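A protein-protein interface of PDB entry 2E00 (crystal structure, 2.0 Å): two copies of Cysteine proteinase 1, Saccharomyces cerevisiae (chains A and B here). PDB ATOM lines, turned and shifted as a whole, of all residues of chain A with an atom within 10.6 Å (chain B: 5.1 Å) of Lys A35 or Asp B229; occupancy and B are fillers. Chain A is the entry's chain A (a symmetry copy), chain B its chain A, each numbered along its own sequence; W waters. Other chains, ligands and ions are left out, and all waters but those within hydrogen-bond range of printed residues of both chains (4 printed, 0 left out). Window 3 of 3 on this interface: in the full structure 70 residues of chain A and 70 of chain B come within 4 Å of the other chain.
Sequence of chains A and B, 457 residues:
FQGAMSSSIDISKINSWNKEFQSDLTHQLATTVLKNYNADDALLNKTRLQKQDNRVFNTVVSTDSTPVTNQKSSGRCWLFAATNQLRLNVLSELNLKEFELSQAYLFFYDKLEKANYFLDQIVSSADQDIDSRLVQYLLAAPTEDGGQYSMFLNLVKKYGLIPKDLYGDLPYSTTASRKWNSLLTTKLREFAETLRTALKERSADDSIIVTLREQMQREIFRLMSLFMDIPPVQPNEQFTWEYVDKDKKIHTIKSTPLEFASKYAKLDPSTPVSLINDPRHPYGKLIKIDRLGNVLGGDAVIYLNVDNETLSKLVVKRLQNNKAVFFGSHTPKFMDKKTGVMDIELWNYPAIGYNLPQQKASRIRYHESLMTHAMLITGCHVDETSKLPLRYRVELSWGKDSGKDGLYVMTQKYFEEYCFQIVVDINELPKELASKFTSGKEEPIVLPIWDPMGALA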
ATOM      1  N   ILE A  14      12.997  -0.860  30.087  1.00  0.00           N
ATOM      2  CA  ILE A  14      13.623  -0.357  28.869  1.00  0.00           C
ATOM      3  C   ILE A  14      12.862   0.803  28.247  1.00  0.00           C
ATOM      4  O   ILE A  14      13.476   1.741  27.751  1.00  0.00           O
ATOM      5  CB  ILE A  14      13.911  -1.474  27.817  1.00  0.00           C
ATOM      6  CG1 ILE A  14      12.624  -2.158  27.350  1.00  0.00           C
ATOM      7  CG2 ILE A  14      14.894  -2.497  28.395  1.00  0.00           C
ATOM      8  CD1 ILE A  14      12.863  -3.200  26.255  1.00  0.00           C
ATOM      9  N   ASN A  15      11.534   0.755  28.286  1.00  0.00           N
ATOM     10  CA  ASN A  15      10.750   1.856  27.736  1.00  0.00           C
ATOM     11  C   ASN A  15      10.869   3.087  28.631  1.00  0.00           C
ATOM     12  O   ASN A  15      10.835   4.221  28.147  1.00  0.00           O
ATOM     13  CB  ASN A  15       9.294   1.451  27.524  1.00  0.00           C
ATOM     14  CG  ASN A  15       9.092   0.692  26.225  1.00  0.00           C
ATOM     15  OD1 ASN A  15       8.925   1.297  25.163  1.00  0.00           O
ATOM     16  ND2 ASN A  15       9.130  -0.635  26.297  1.00  0.00           N
ATOM     17  N   ASN A  18      14.220   4.501  27.894  1.00  0.00           N
ATOM     18  CA  ASN A  18      14.149   5.153  26.590  1.00  0.00           C
ATOM     19  C   ASN A  18      13.636   6.583  26.717  1.00  0.00           C
ATOM     20  O   ASN A  18      14.198   7.501  26.112  1.00  0.00           O
ATOM     21  CB  ASN A  18      13.259   4.368  25.626  1.00  0.00           C
ATOM     22  CG  ASN A  18      13.293   4.930  24.222  1.00  0.00           C
ATOM     23  OD1 ASN A  18      14.353   4.988  23.594  1.00  0.00           O
ATOM     24  ND2 ASN A  18      12.141   5.373  23.726  1.00  0.00           N
ATOM     25  N   LYS A  19      12.571   6.768  27.497  1.00  0.00           N
ATOM     26  CA  LYS A  19      12.008   8.101  27.705  1.00  0.00           C
ATOM     27  C   LYS A  19      13.070   9.017  28.308  1.00  0.00           C
ATOM     28  O   LYS A  19      13.252  10.158  27.858  1.00  0.00           O
ATOM     29  CB  LYS A  19      10.787   8.044  28.630  1.00  0.00           C
ATOM     30  CG  LYS A  19      10.107   9.394  28.807  1.00  0.00           C
ATOM     31  CD  LYS A  19       8.913   9.308  29.753  1.00  0.00           C
ATOM     32  CE  LYS A  19       8.247  10.668  29.919  1.00  0.00           C
ATOM     33  NZ  LYS A  19       7.114  10.605  30.883  1.00  0.00           N
ATOM     34  N   PHE A  21      16.422   8.734  28.166  1.00  0.00           N
ATOM     35  CA  PHE A  21      17.457   9.006  27.168  1.00  0.00           C
ATOM     36  C   PHE A  21      16.996  10.012  26.113  1.00  0.00           C
ATOM     37  O   PHE A  21      17.747  10.919  25.745  1.00  0.00           O
ATOM     38  CB  PHE A  21      17.913   7.703  26.496  1.00  0.00           C
ATOM     39  CG  PHE A  21      18.543   6.713  27.444  1.00  0.00           C
ATOM     40  CD1 PHE A  21      19.280   7.147  28.541  1.00  0.00           C
ATOM     41  CD2 PHE A  21      18.392   5.344  27.239  1.00  0.00           C
ATOM     42  CE1 PHE A  21      19.852   6.234  29.426  1.00  0.00           C
ATOM     43  CE2 PHE A  21      18.960   4.425  28.117  1.00  0.00           C
ATOM     44  CZ  PHE A  21      19.688   4.869  29.210  1.00  0.00           C
ATOM     45  N   GLN A  22      15.749   9.880  25.663  1.00  0.00           N
ATOM     46  CA  GLN A  22      15.193  10.782  24.653  1.00  0.00           C
ATOM     47  C   GLN A  22      15.058  12.234  25.114  1.00  0.00           C
ATOM     48  O   GLN A  22      14.914  13.134  24.285  1.00  0.00           O
ATOM     49  CB  GLN A  22      13.842  10.267  24.144  1.00  0.00           C
ATOM     50  CG  GLN A  22      13.934   9.089  23.171  1.00  0.00           C
ATOM     51  CD  GLN A  22      14.616   9.450  21.856  1.00  0.00           C
ATOM     52  OE1 GLN A  22      15.404   8.669  21.314  1.00  0.00           O
ATOM     53  NE2 GLN A  22      14.303  10.631  21.330  1.00  0.00           N
ATOM     54  N   THR A  26      21.946  15.348  23.600  1.00  0.00           N
ATOM     55  CA  THR A  26      23.094  14.668  23.010  1.00  0.00           C
ATOM     56  C   THR A  26      22.649  13.306  22.476  1.00  0.00           C
ATOM     57  O   THR A  26      23.006  12.922  21.366  1.00  0.00           O
ATOM     58  CB  THR A  26      24.243  14.518  24.025  1.00  0.00           C
ATOM     59  OG1 THR A  26      24.568  15.810  24.555  1.00  0.00           O
ATOM     60  CG2 THR A  26      25.492  13.929  23.355  1.00  0.00           C
ATOM     61  N   HIS A  27      21.812  12.616  23.249  1.00  0.00           N
ATOM     62  CA  HIS A  27      21.290  11.313  22.855  1.00  0.00           C
ATOM     63  C   HIS A  27      20.398  11.439  21.611  1.00  0.00           C
ATOM     64  O   HIS A  27      20.479  10.612  20.699  1.00  0.00           O
ATOM     65  CB  HIS A  27      20.492  10.684  24.003  1.00  0.00           C
ATOM     66  CG  HIS A  27      20.122   9.256  23.761  1.00  0.00           C
ATOM     67  ND1 HIS A  27      20.916   8.205  24.166  1.00  0.00           N
ATOM     68  CD2 HIS A  27      19.048   8.702  23.147  1.00  0.00           C
ATOM     69  CE1 HIS A  27      20.349   7.066  23.814  1.00  0.00           C
ATOM     70  NE2 HIS A  27      19.215   7.340  23.194  1.00  0.00           N
ATOM     71  N   GLN A  28      19.546  12.466  21.585  1.00  0.00           N
ATOM     72  CA  GLN A  28      18.660  12.694  20.442  1.00  0.00           C
ATOM     73  C   GLN A  28      19.500  12.847  19.179  1.00  0.00           C
ATOM     74  O   GLN A  28      19.194  12.257  18.146  1.00  0.00           O
ATOM     75  CB  GLN A  28      17.812  13.953  20.640  1.00  0.00           C
ATOM     76  CG  GLN A  28      16.713  13.827  21.682  1.00  0.00           C
ATOM     77  CD  GLN A  28      15.940  15.121  21.853  1.00  0.00           C
ATOM     78  OE1 GLN A  28      15.412  15.675  20.887  1.00  0.00           O
ATOM     79  NE2 GLN A  28      15.884  15.620  23.086  1.00  0.00           N
ATOM     80  N   LEU A  29      20.562  13.641  19.285  1.00  0.00           N
ATOM     81  CA  LEU A  29      21.466  13.873  18.162  1.00  0.00           C
ATOM     82  C   LEU A  29      22.194  12.592  17.757  1.00  0.00           C
ATOM     83  O   LEU A  29      22.253  12.244  16.575  1.00  0.00           O
ATOM     84  CB  LEU A  29      22.483  14.960  18.521  1.00  0.00           C
ATOM     85  CG  LEU A  29      23.498  15.310  17.423  1.00  0.00           C
ATOM     86  CD1 LEU A  29      22.793  15.616  16.103  1.00  0.00           C
ATOM     87  CD2 LEU A  29      24.342  16.497  17.868  1.00  0.00           C
ATOM     88  N   ALA A  30      22.745  11.896  18.749  1.00  0.00           N
ATOM     89  CA  ALA A  30      23.478  10.662  18.520  1.00  0.00           C
ATOM     90  C   ALA A  30      22.661   9.583  17.807  1.00  0.00           C
ATOM     91  O   ALA A  30      23.134   8.993  16.837  1.00  0.00           O
ATOM     92  CB  ALA A  30      24.026  10.125  19.846  1.00  0.00           C
ATOM     93  N   THR A  31      21.442   9.327  18.272  1.00  0.00           N
ATOM     94  CA  THR A  31      20.614   8.298  17.645  1.00  0.00           C
ATOM     95  C   THR A  31      20.177   8.668  16.230  1.00  0.00           C
ATOM     96  O   THR A  31      20.016   7.792  15.375  1.00  0.00           O
ATOM     97  CB  THR A  31      19.386   7.915  18.513  1.00  0.00           C
ATOM     98  OG1 THR A  31      18.719   6.793  17.915  1.00  0.00           O
ATOM     99  CG2 THR A  31      18.422   9.086  18.651  1.00  0.00           C
ATOM    100  N   THR A  32      20.012   9.962  15.969  1.00  0.00           N
ATOM    101  CA  THR A  32      19.623  10.410  14.634  1.00  0.00           C
ATOM    102  C   THR A  32      20.759  10.087  13.653  1.00  0.00           C
ATOM    103  O   THR A  32      20.554   9.421  12.642  1.00  0.00           O
ATOM    104  CB  THR A  32      19.351  11.936  14.598  1.00  0.00           C
ATOM    105  OG1 THR A  32      18.304  12.260  15.520  1.00  0.00           O
ATOM    106  CG2 THR A  32      18.933  12.372  13.199  1.00  0.00           C
ATOM    107  N   VAL A  33      21.967  10.516  14.003  1.00  0.00           N
ATOM    108  CA  VAL A  33      23.147  10.305  13.162  1.00  0.00           C
ATOM    109  C   VAL A  33      23.559   8.830  13.051  1.00  0.00           C
ATOM    110  O   VAL A  33      23.821   8.326  11.949  1.00  0.00           O
ATOM    111  CB  VAL A  33      24.340  11.149  13.684  1.00  0.00           C
ATOM    112  CG1 VAL A  33      25.597  10.891  12.860  1.00  0.00           C
ATOM    113  CG2 VAL A  33      23.985  12.630  13.642  1.00  0.00           C
ATOM    114  N   LEU A  34      23.569   8.129  14.181  1.00  0.00           N
ATOM    115  CA  LEU A  34      23.976   6.725  14.210  1.00  0.00           C
ATOM    116  C   LEU A  34      23.067   5.725  13.495  1.00  0.00           C
ATOM    117  O   LEU A  34      23.442   4.563  13.321  1.00  0.00           O
ATOM    118  CB  LEU A  34      24.285   6.282  15.639  1.00  0.00           C
ATOM    119  CG  LEU A  34      25.743   6.324  16.128  1.00  0.00           C
ATOM    120  CD1 LEU A  34      26.668   7.056  15.169  1.00  0.00           C
ATOM    121  CD2 LEU A  34      25.797   6.928  17.521  1.00  0.00           C
ATOM    122  N   LYS A  35      21.867   6.155  13.114  1.00  0.00           N
ATOM    123  CA  LYS A  35      20.965   5.288  12.357  1.00  0.00           C
ATOM    124  C   LYS A  35      21.243   5.531  10.869  1.00  0.00           C
ATOM    125  O   LYS A  35      20.842   4.742  10.014  1.00  0.00           O
ATOM    126  CB  LYS A  35      19.486   5.595  12.657  1.00  0.00           C
ATOM    127  CG  LYS A  35      18.989   5.111  14.025  1.00  0.00           C
ATOM    128  CD  LYS A  35      17.450   5.094  14.115  1.00  0.00           C
ATOM    129  CE  LYS A  35      16.827   6.493  14.224  1.00  0.00           C
ATOM    130  NZ  LYS A  35      16.997   7.114  15.579  1.00  0.00           N
ATOM    131  N   ASN A  36      21.942   6.623  10.571  1.00  0.00           N
ATOM    132  CA  ASN A  36      22.256   6.993   9.190  1.00  0.00           C
ATOM    133  C   ASN A  36      23.603   6.528   8.652  1.00  0.00           C
ATOM    134  O   ASN A  36      23.698   6.151   7.486  1.00  0.00           O
ATOM    135  CB  ASN A  36      22.144   8.512   9.008  1.00  0.00           C
ATOM    136  CG  ASN A  36      20.731   9.024   9.215  1.00  0.00           C
ATOM    137  OD1 ASN A  36      19.774   8.261   9.152  1.00  0.00           O
ATOM    138  ND2 ASN A  36      20.596  10.324   9.471  1.00  0.00           N
ATOM    139  N   TYR A  37      24.643   6.569   9.483  1.00  0.00           N
ATOM    140  CA  TYR A  37      25.984   6.183   9.044  1.00  0.00           C
ATOM    141  C   TYR A  37      26.761   5.311  10.018  1.00  0.00           C
ATOM    142  O   TYR A  37      26.451   5.260  11.205  1.00  0.00           O
ATOM    143  CB  TYR A  37      26.810   7.444   8.719  1.00  0.00           C
ATOM    144  CG  TYR A  37      26.228   8.214   7.554  1.00  0.00           C
ATOM    145  CD1 TYR A  37      26.198   7.646   6.279  1.00  0.00           C
ATOM    146  CD2 TYR A  37      25.576   9.434   7.748  1.00  0.00           C
ATOM    147  CE1 TYR A  37      25.523   8.253   5.230  1.00  0.00           C
ATOM    148  CE2 TYR A  37      24.894  10.058   6.696  1.00  0.00           C
ATOM    149  CZ  TYR A  37      24.868   9.452   5.440  1.00  0.00           C
ATOM    150  OH  TYR A  37      24.162  10.012   4.396  1.00  0.00           O
ATOM    151  N   ASN A  38      27.762   4.616   9.479  1.00  0.00           N
ATOM    152  CA  ASN A  38      28.660   3.758  10.247  1.00  0.00           C
ATOM    153  C   ASN A  38      29.255   4.637  11.347  1.00  0.00           C
ATOM    154  O   ASN A  38      29.624   5.783  11.090  1.00  0.00           O
ATOM    155  CB  ASN A  38      29.762   3.225   9.318  1.00  0.00           C
ATOM    156  CG  ASN A  38      30.851   2.472  10.058  1.00  0.00           C
ATOM    157  OD1 ASN A  38      30.879   1.237  10.065  1.00  0.00           O
ATOM    158  ND2 ASN A  38      31.769   3.213  10.666  1.00  0.00           N
ATOM    159  N   ALA A  39      29.346   4.100  12.561  1.00  0.00           N
ATOM    160  CA  ALA A  39      29.856   4.853  13.707  1.00  0.00           C
ATOM    161  C   ALA A  39      31.239   5.476  13.516  1.00  0.00           C
ATOM    162  O   ALA A  39      31.477   6.597  13.963  1.00  0.00           O
ATOM    163  CB  ALA A  39      29.822   3.993  14.966  1.00  0.00           C
ATOM    164  N   ASP A  40      32.148   4.754  12.865  1.00  0.00           N
ATOM    165  CA  ASP A  40      33.491   5.270  12.608  1.00  0.00           C
ATOM    166  C   ASP A  40      33.453   6.427  11.606  1.00  0.00           C
ATOM    167  O   ASP A  40      34.194   7.402  11.745  1.00  0.00           O
ATOM    168  CB  ASP A  40      34.425   4.156  12.106  1.00  0.00           C
ATOM    169  CG  ASP A  40      34.894   3.227  13.229  1.00  0.00           C
ATOM    170  OD1 ASP A  40      34.876   3.633  14.413  1.00  0.00           O
ATOM    171  OD2 ASP A  40      35.287   2.084  12.926  1.00  0.00           O
ATOM    172  N   ALA A  42      30.832   8.421  11.073  1.00  0.00           N
ATOM    173  CA  ALA A  42      30.163   9.523  11.748  1.00  0.00           C
ATOM    174  C   ALA A  42      31.041  10.219  12.773  1.00  0.00           C
ATOM    175  O   ALA A  42      31.106  11.444  12.809  1.00  0.00           O
ATOM    176  CB  ALA A  42      28.888   9.022  12.431  1.00  0.00           C
ATOM    177  N   LEU A  43      31.737   9.433  13.586  1.00  0.00           N
ATOM    178  CA  LEU A  43      32.554   9.985  14.662  1.00  0.00           C
ATOM    179  C   LEU A  43      34.004  10.358  14.410  1.00  0.00           C
ATOM    180  O   LEU A  43      34.676  10.826  15.332  1.00  0.00           O
ATOM    181  CB  LEU A  43      32.454   9.086  15.892  1.00  0.00           C
ATOM    182  CG  LEU A  43      31.015   8.908  16.389  1.00  0.00           C
ATOM    183  CD1 LEU A  43      30.980   7.886  17.501  1.00  0.00           C
ATOM    184  CD2 LEU A  43      30.453  10.246  16.864  1.00  0.00           C
ATOM    185  N   ILE A 352      29.511  10.420  22.532  1.00  0.00           N
ATOM    186  CA  ILE A 352      28.262   9.664  22.667  1.00  0.00           C
ATOM    187  C   ILE A 352      28.324   8.831  23.950  1.00  0.00           C
ATOM    188  O   ILE A 352      27.638   7.817  24.075  1.00  0.00           O
ATOM    189  CB  ILE A 352      27.978   8.717  21.471  1.00  0.00           C
ATOM    190  CG1 ILE A 352      29.099   7.689  21.314  1.00  0.00           C
ATOM    191  CG2 ILE A 352      27.788   9.519  20.181  1.00  0.00           C
ATOM    192  CD1 ILE A 352      28.741   6.543  20.399  1.00  0.00           C
ATOM    193  N   PHE B 108      16.064  -6.424  16.881  1.00  0.00           N
ATOM    194  CA  PHE B 108      16.348  -5.520  17.998  1.00  0.00           C
ATOM    195  C   PHE B 108      16.263  -6.253  19.339  1.00  0.00           C
ATOM    196  O   PHE B 108      17.205  -6.239  20.129  1.00  0.00           O
ATOM    197  CB  PHE B 108      15.371  -4.337  18.000  1.00  0.00           C
ATOM    198  CG  PHE B 108      15.648  -3.323  19.084  1.00  0.00           C
ATOM    199  CD1 PHE B 108      16.553  -2.289  18.868  1.00  0.00           C
ATOM    200  CD2 PHE B 108      15.026  -3.417  20.325  1.00  0.00           C
ATOM    201  CE1 PHE B 108      16.838  -1.364  19.873  1.00  0.00           C
ATOM    202  CE2 PHE B 108      15.306  -2.497  21.339  1.00  0.00           C
ATOM    203  CZ  PHE B 108      16.213  -1.471  21.115  1.00  0.00           C
ATOM    204  N   TYR B 167       7.892  -0.828  11.302  1.00  0.00           N
ATOM    205  CA  TYR B 167       9.271  -0.849  11.790  1.00  0.00           C
ATOM    206  C   TYR B 167      10.107  -1.654  10.789  1.00  0.00           C
ATOM    207  O   TYR B 167      10.076  -2.881  10.801  1.00  0.00           O
ATOM    208  CB  TYR B 167       9.261  -1.530  13.170  1.00  0.00           C
ATOM    209  CG  TYR B 167      10.540  -1.470  13.970  1.00  0.00           C
ATOM    210  CD1 TYR B 167      10.911  -0.307  14.646  1.00  0.00           C
ATOM    211  CD2 TYR B 167      11.354  -2.593  14.091  1.00  0.00           C
ATOM    212  CE1 TYR B 167      12.066  -0.270  15.433  1.00  0.00           C
ATOM    213  CE2 TYR B 167      12.508  -2.570  14.868  1.00  0.00           C
ATOM    214  CZ  TYR B 167      12.862  -1.412  15.536  1.00  0.00           C
ATOM    215  OH  TYR B 167      14.004  -1.404  16.308  1.00  0.00           O
ATOM    216  N   LEU B 170      15.302   0.446   8.124  1.00  0.00           N
ATOM    217  CA  LEU B 170      15.822   1.787   7.867  1.00  0.00           C
ATOM    218  C   LEU B 170      17.220   2.051   8.438  1.00  0.00           C
ATOM    219  O   LEU B 170      18.099   2.528   7.722  1.00  0.00           O
ATOM    220  CB  LEU B 170      14.848   2.858   8.366  1.00  0.00           C
ATOM    221  CG  LEU B 170      13.501   2.962   7.655  1.00  0.00           C
ATOM    222  CD1 LEU B 170      12.733   4.160   8.193  1.00  0.00           C
ATOM    223  CD2 LEU B 170      13.711   3.094   6.154  1.00  0.00           C
ATOM    224  N   PRO B 171      17.451   1.711   9.723  1.00  0.00           N
ATOM    225  CA  PRO B 171      18.763   1.941  10.343  1.00  0.00           C
ATOM    226  C   PRO B 171      19.929   1.243   9.647  1.00  0.00           C
ATOM    227  O   PRO B 171      19.817   0.095   9.214  1.00  0.00           O
ATOM    228  CB  PRO B 171      18.571   1.400  11.766  1.00  0.00           C
ATOM    229  CG  PRO B 171      17.098   1.608  12.016  1.00  0.00           C
ATOM    230  CD  PRO B 171      16.503   1.155  10.710  1.00  0.00           C
ATOM    231  N   TYR B 172      21.050   1.956   9.562  1.00  0.00           N
ATOM    232  CA  TYR B 172      22.279   1.445   8.953  1.00  0.00           C
ATOM    233  C   TYR B 172      22.684   0.090   9.535  1.00  0.00           C
ATOM    234  O   TYR B 172      23.059  -0.817   8.794  1.00  0.00           O
ATOM    235  CB  TYR B 172      23.430   2.446   9.179  1.00  0.00           C
ATOM    236  CG  TYR B 172      24.797   1.927   8.770  1.00  0.00           C
ATOM    237  CD1 TYR B 172      25.227   2.008   7.443  1.00  0.00           C
ATOM    238  CD2 TYR B 172      25.644   1.320   9.701  1.00  0.00           C
ATOM    239  CE1 TYR B 172      26.468   1.491   7.051  1.00  0.00           C
ATOM    240  CE2 TYR B 172      26.880   0.799   9.323  1.00  0.00           C
ATOM    241  CZ  TYR B 172      27.286   0.886   7.994  1.00  0.00           C
ATOM    242  OH  TYR B 172      28.502   0.357   7.615  1.00  0.00           O
ATOM    243  N   SER B 225      20.025   1.761  21.659  1.00  0.00           N
ATOM    244  CA  SER B 225      19.064   2.760  21.201  1.00  0.00           C
ATOM    245  C   SER B 225      19.700   3.815  20.296  1.00  0.00           C
ATOM    246  O   SER B 225      19.003   4.603  19.663  1.00  0.00           O
ATOM    247  CB  SER B 225      18.352   3.426  22.385  1.00  0.00           C
ATOM    248  OG  SER B 225      19.219   4.294  23.078  1.00  0.00           O
ATOM    249  N   LEU B 226      21.028   3.846  20.258  1.00  0.00           N
ATOM    250  CA  LEU B 226      21.738   4.794  19.411  1.00  0.00           C
ATOM    251  C   LEU B 226      21.785   4.296  17.973  1.00  0.00           C
ATOM    252  O   LEU B 226      21.830   5.098  17.044  1.00  0.00           O
ATOM    253  CB  LEU B 226      23.173   5.008  19.906  1.00  0.00           C
ATOM    254  CG  LEU B 226      23.356   5.639  21.285  1.00  0.00           C
ATOM    255  CD1 LEU B 226      24.838   5.754  21.590  1.00  0.00           C
ATOM    256  CD2 LEU B 226      22.685   7.008  21.323  1.00  0.00           C
ATOM    257  N   PHE B 227      21.759   2.975  17.797  1.00  0.00           N
ATOM    258  CA  PHE B 227      21.834   2.374  16.467  1.00  0.00           C
ATOM    259  C   PHE B 227      20.505   1.906  15.880  1.00  0.00           C
ATOM    260  O   PHE B 227      20.396   1.719  14.670  1.00  0.00           O
ATOM    261  CB  PHE B 227      22.875   1.252  16.466  1.00  0.00           C
ATOM    262  CG  PHE B 227      24.248   1.713  16.885  1.00  0.00           C
ATOM    263  CD1 PHE B 227      24.546   1.915  18.231  1.00  0.00           C
ATOM    264  CD2 PHE B 227      25.227   1.992  15.934  1.00  0.00           C
ATOM    265  CE1 PHE B 227      25.797   2.395  18.622  1.00  0.00           C
ATOM    266  CE2 PHE B 227      26.478   2.469  16.317  1.00  0.00           C
ATOM    267  CZ  PHE B 227      26.764   2.672  17.663  1.00  0.00           C
ATOM    268  N   MET B 228      19.514   1.697  16.747  1.00  0.00           N
ATOM    269  CA  MET B 228      18.159   1.298  16.355  1.00  0.00           C
ATOM    270  C   MET B 228      17.202   1.841  17.416  1.00  0.00           C
ATOM    271  O   MET B 228      17.579   1.972  18.580  1.00  0.00           O
ATOM    272  CB  MET B 228      18.001  -0.229  16.295  1.00  0.00           C
ATOM    273  CG  MET B 228      18.598  -0.904  15.065  1.00  0.00           C
ATOM    274  SD  MET B 228      18.230  -2.676  15.007  1.00  0.00           S
ATOM    275  CE  MET B 228      16.530  -2.645  14.413  1.00  0.00           C
ATOM    276  N   ASP B 229      15.984   2.195  17.017  1.00  0.00           N
ATOM    277  CA  ASP B 229      15.014   2.691  17.989  1.00  0.00           C
ATOM    278  C   ASP B 229      14.299   1.501  18.602  1.00  0.00           C
ATOM    279  O   ASP B 229      14.114   0.476  17.947  1.00  0.00           O
ATOM    280  CB  ASP B 229      13.944   3.569  17.332  1.00  0.00           C
ATOM    281  CG  ASP B 229      14.514   4.781  16.621  1.00  0.00           C
ATOM    282  OD1 ASP B 229      15.425   5.446  17.156  1.00  0.00           O
ATOM    283  OD2 ASP B 229      14.012   5.083  15.524  1.00  0.00           O
ATOM    284  N   ILE B 230      13.882   1.634  19.853  1.00  0.00           N
ATOM    285  CA  ILE B 230      13.114   0.567  20.480  1.00  0.00           C
ATOM    286  C   ILE B 230      11.811   0.606  19.658  1.00  0.00           C
ATOM    287  O   ILE B 230      11.433   1.668  19.161  1.00  0.00           O
ATOM    288  CB  ILE B 230      12.828   0.877  21.985  1.00  0.00           C
ATOM    289  CG1 ILE B 230      12.135  -0.315  22.654  1.00  0.00           C
ATOM    290  CG2 ILE B 230      11.979   2.142  22.131  1.00  0.00           C
ATOM    291  CD1 ILE B 230      12.016  -0.191  24.155  1.00  0.00           C
ATOM    292  N   PRO B 231      11.212  -0.559  19.361  1.00  0.00           N
ATOM    293  CA  PRO B 231       9.963  -0.581  18.584  1.00  0.00           C
ATOM    294  C   PRO B 231       8.944   0.436  19.122  1.00  0.00           C
ATOM    295  O   PRO B 231       8.919   0.720  20.320  1.00  0.00           O
ATOM    296  CB  PRO B 231       9.507  -2.022  18.742  1.00  0.00           C
ATOM    297  CG  PRO B 231      10.829  -2.759  18.680  1.00  0.00           C
ATOM    298  CD  PRO B 231      11.699  -1.930  19.610  1.00  0.00           C
HETATM  299  O   HOH W   1       7.744   0.431  22.734  1.00  0.00           O
HETATM  300  O   HOH W   2      14.730   4.000  21.094  1.00  0.00           O
HETATM  301  O   HOH W   3      22.337   2.001  12.865  1.00  0.00           O
HETATM  302  O   HOH W   4      16.546   5.434  19.645  1.00  0.00           O
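Water W4 lies within hydrogen-bond range of O of Ser B225 (2.6 Å), OD1 of Asp B229 (2.7 Å) and OG1 of Thr A31 (3.1 Å). Water W3 lies within hydrogen-bond range of the backbone carbonyl oxygen of Phe B227 (2.7 Å) and the backbone carbonyl oxygen of Leu A34 (2.8 Å).
The backbone NH (N) of Tyr B172 is in hydrogen-bond range of the backbone carbonyl oxygen (O) of Lys A35, 2.8 Å away. The side-chain hydroxyl (OG) of Ser B225 sits at hydrogen-bond distance from a ring nitrogen (NE2) of His A27 (3.0 Å). The backbone carbonyl oxygen (O) of Ser B225 sits at hydrogen-bond distance from the side-chain hydroxyl (OG1) of Thr A31 (2.8 Å). OD1 of Asp B229 lies within salt-bridge range of NZ of Lys A35 (2.8 Å).
OH of Tyr B167 lies within hydrogen-bond range of O of Asp B229 (2.5 Å). NZ of Lys A35 lies within hydrogen-bond range of OG1 of Thr A31 (2.9 Å). The backbone NH (N) of Asp A40 sits close to the side-chain amide nitrogen (ND2) of Asn A38 (2.7 Å).
Ile B230 touches Asn A15 (CD1 to OD1, 3.6 Å). Ile B230 touches Asn A18. His A27 touches Leu B226 (CE1 to CD2, 3.4 Å). Ala A30 touches Leu B226. Thr A31 touches Leu B226. Leu B226 touches Leu A34 (O to CB, 3.1 Å). Phe B227 touches Leu A34. Phe B227 touches Lys A35 (O to CG, 3.7 Å). Asn A38 touches Tyr B172. Phe B227 touches Ala A39.
Lys A35 touches just these residues of chain B: Pro B171, Tyr B172, Phe B227 and Asp B229. Asp B229 touches just these residues of chain A: Thr A31 (3.6 Å) and Lys A35 (2.8 Å). Pro B171 touches one residue of chain A. No residue of chain A comes within 4 Å of Pro B231. Of the printed residues of chain B, Asn A18 touches Ile B230. Of the printed residues of chain A, Leu B226 touches His A27, Ala A30, Thr A31 and Leu A34. Of the printed residues of chain A, Ser B225 touches His A27 (3.0 Å) and Thr A31 (2.8 Å). Printed residues of chain B within 4 Å of His A27: Ser B225 (3.0 Å) and Leu B226 (3.4 Å). Leu B170 touches none of the printed residues of chain A. The nearest residue of chain B that does not touch Lys A35 is Leu B226 (4.1 Å). The nearest printed residue of chain B that does not touch Asn A15 is Pro B231 (4.9 Å).
No position is printed for both chains.
Hydrophobic or aromatic side chains of chain B within 4 Å of the printed part of chain A: Tyr B172, Leu B226, Phe B227 and Ile B230. Hydrophobic or aromatic side chains of chain A within 4 Å of the printed part of chain B: Ile A14, His A27, Ala A30, Leu A34 and Ala A39. Among the printed residues, Asp or Glu carboxylates within 4 Å of a Lys or Arg side-chain nitrogen of the other chain: Lys A35 with Asp B229 (2.8 Å).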
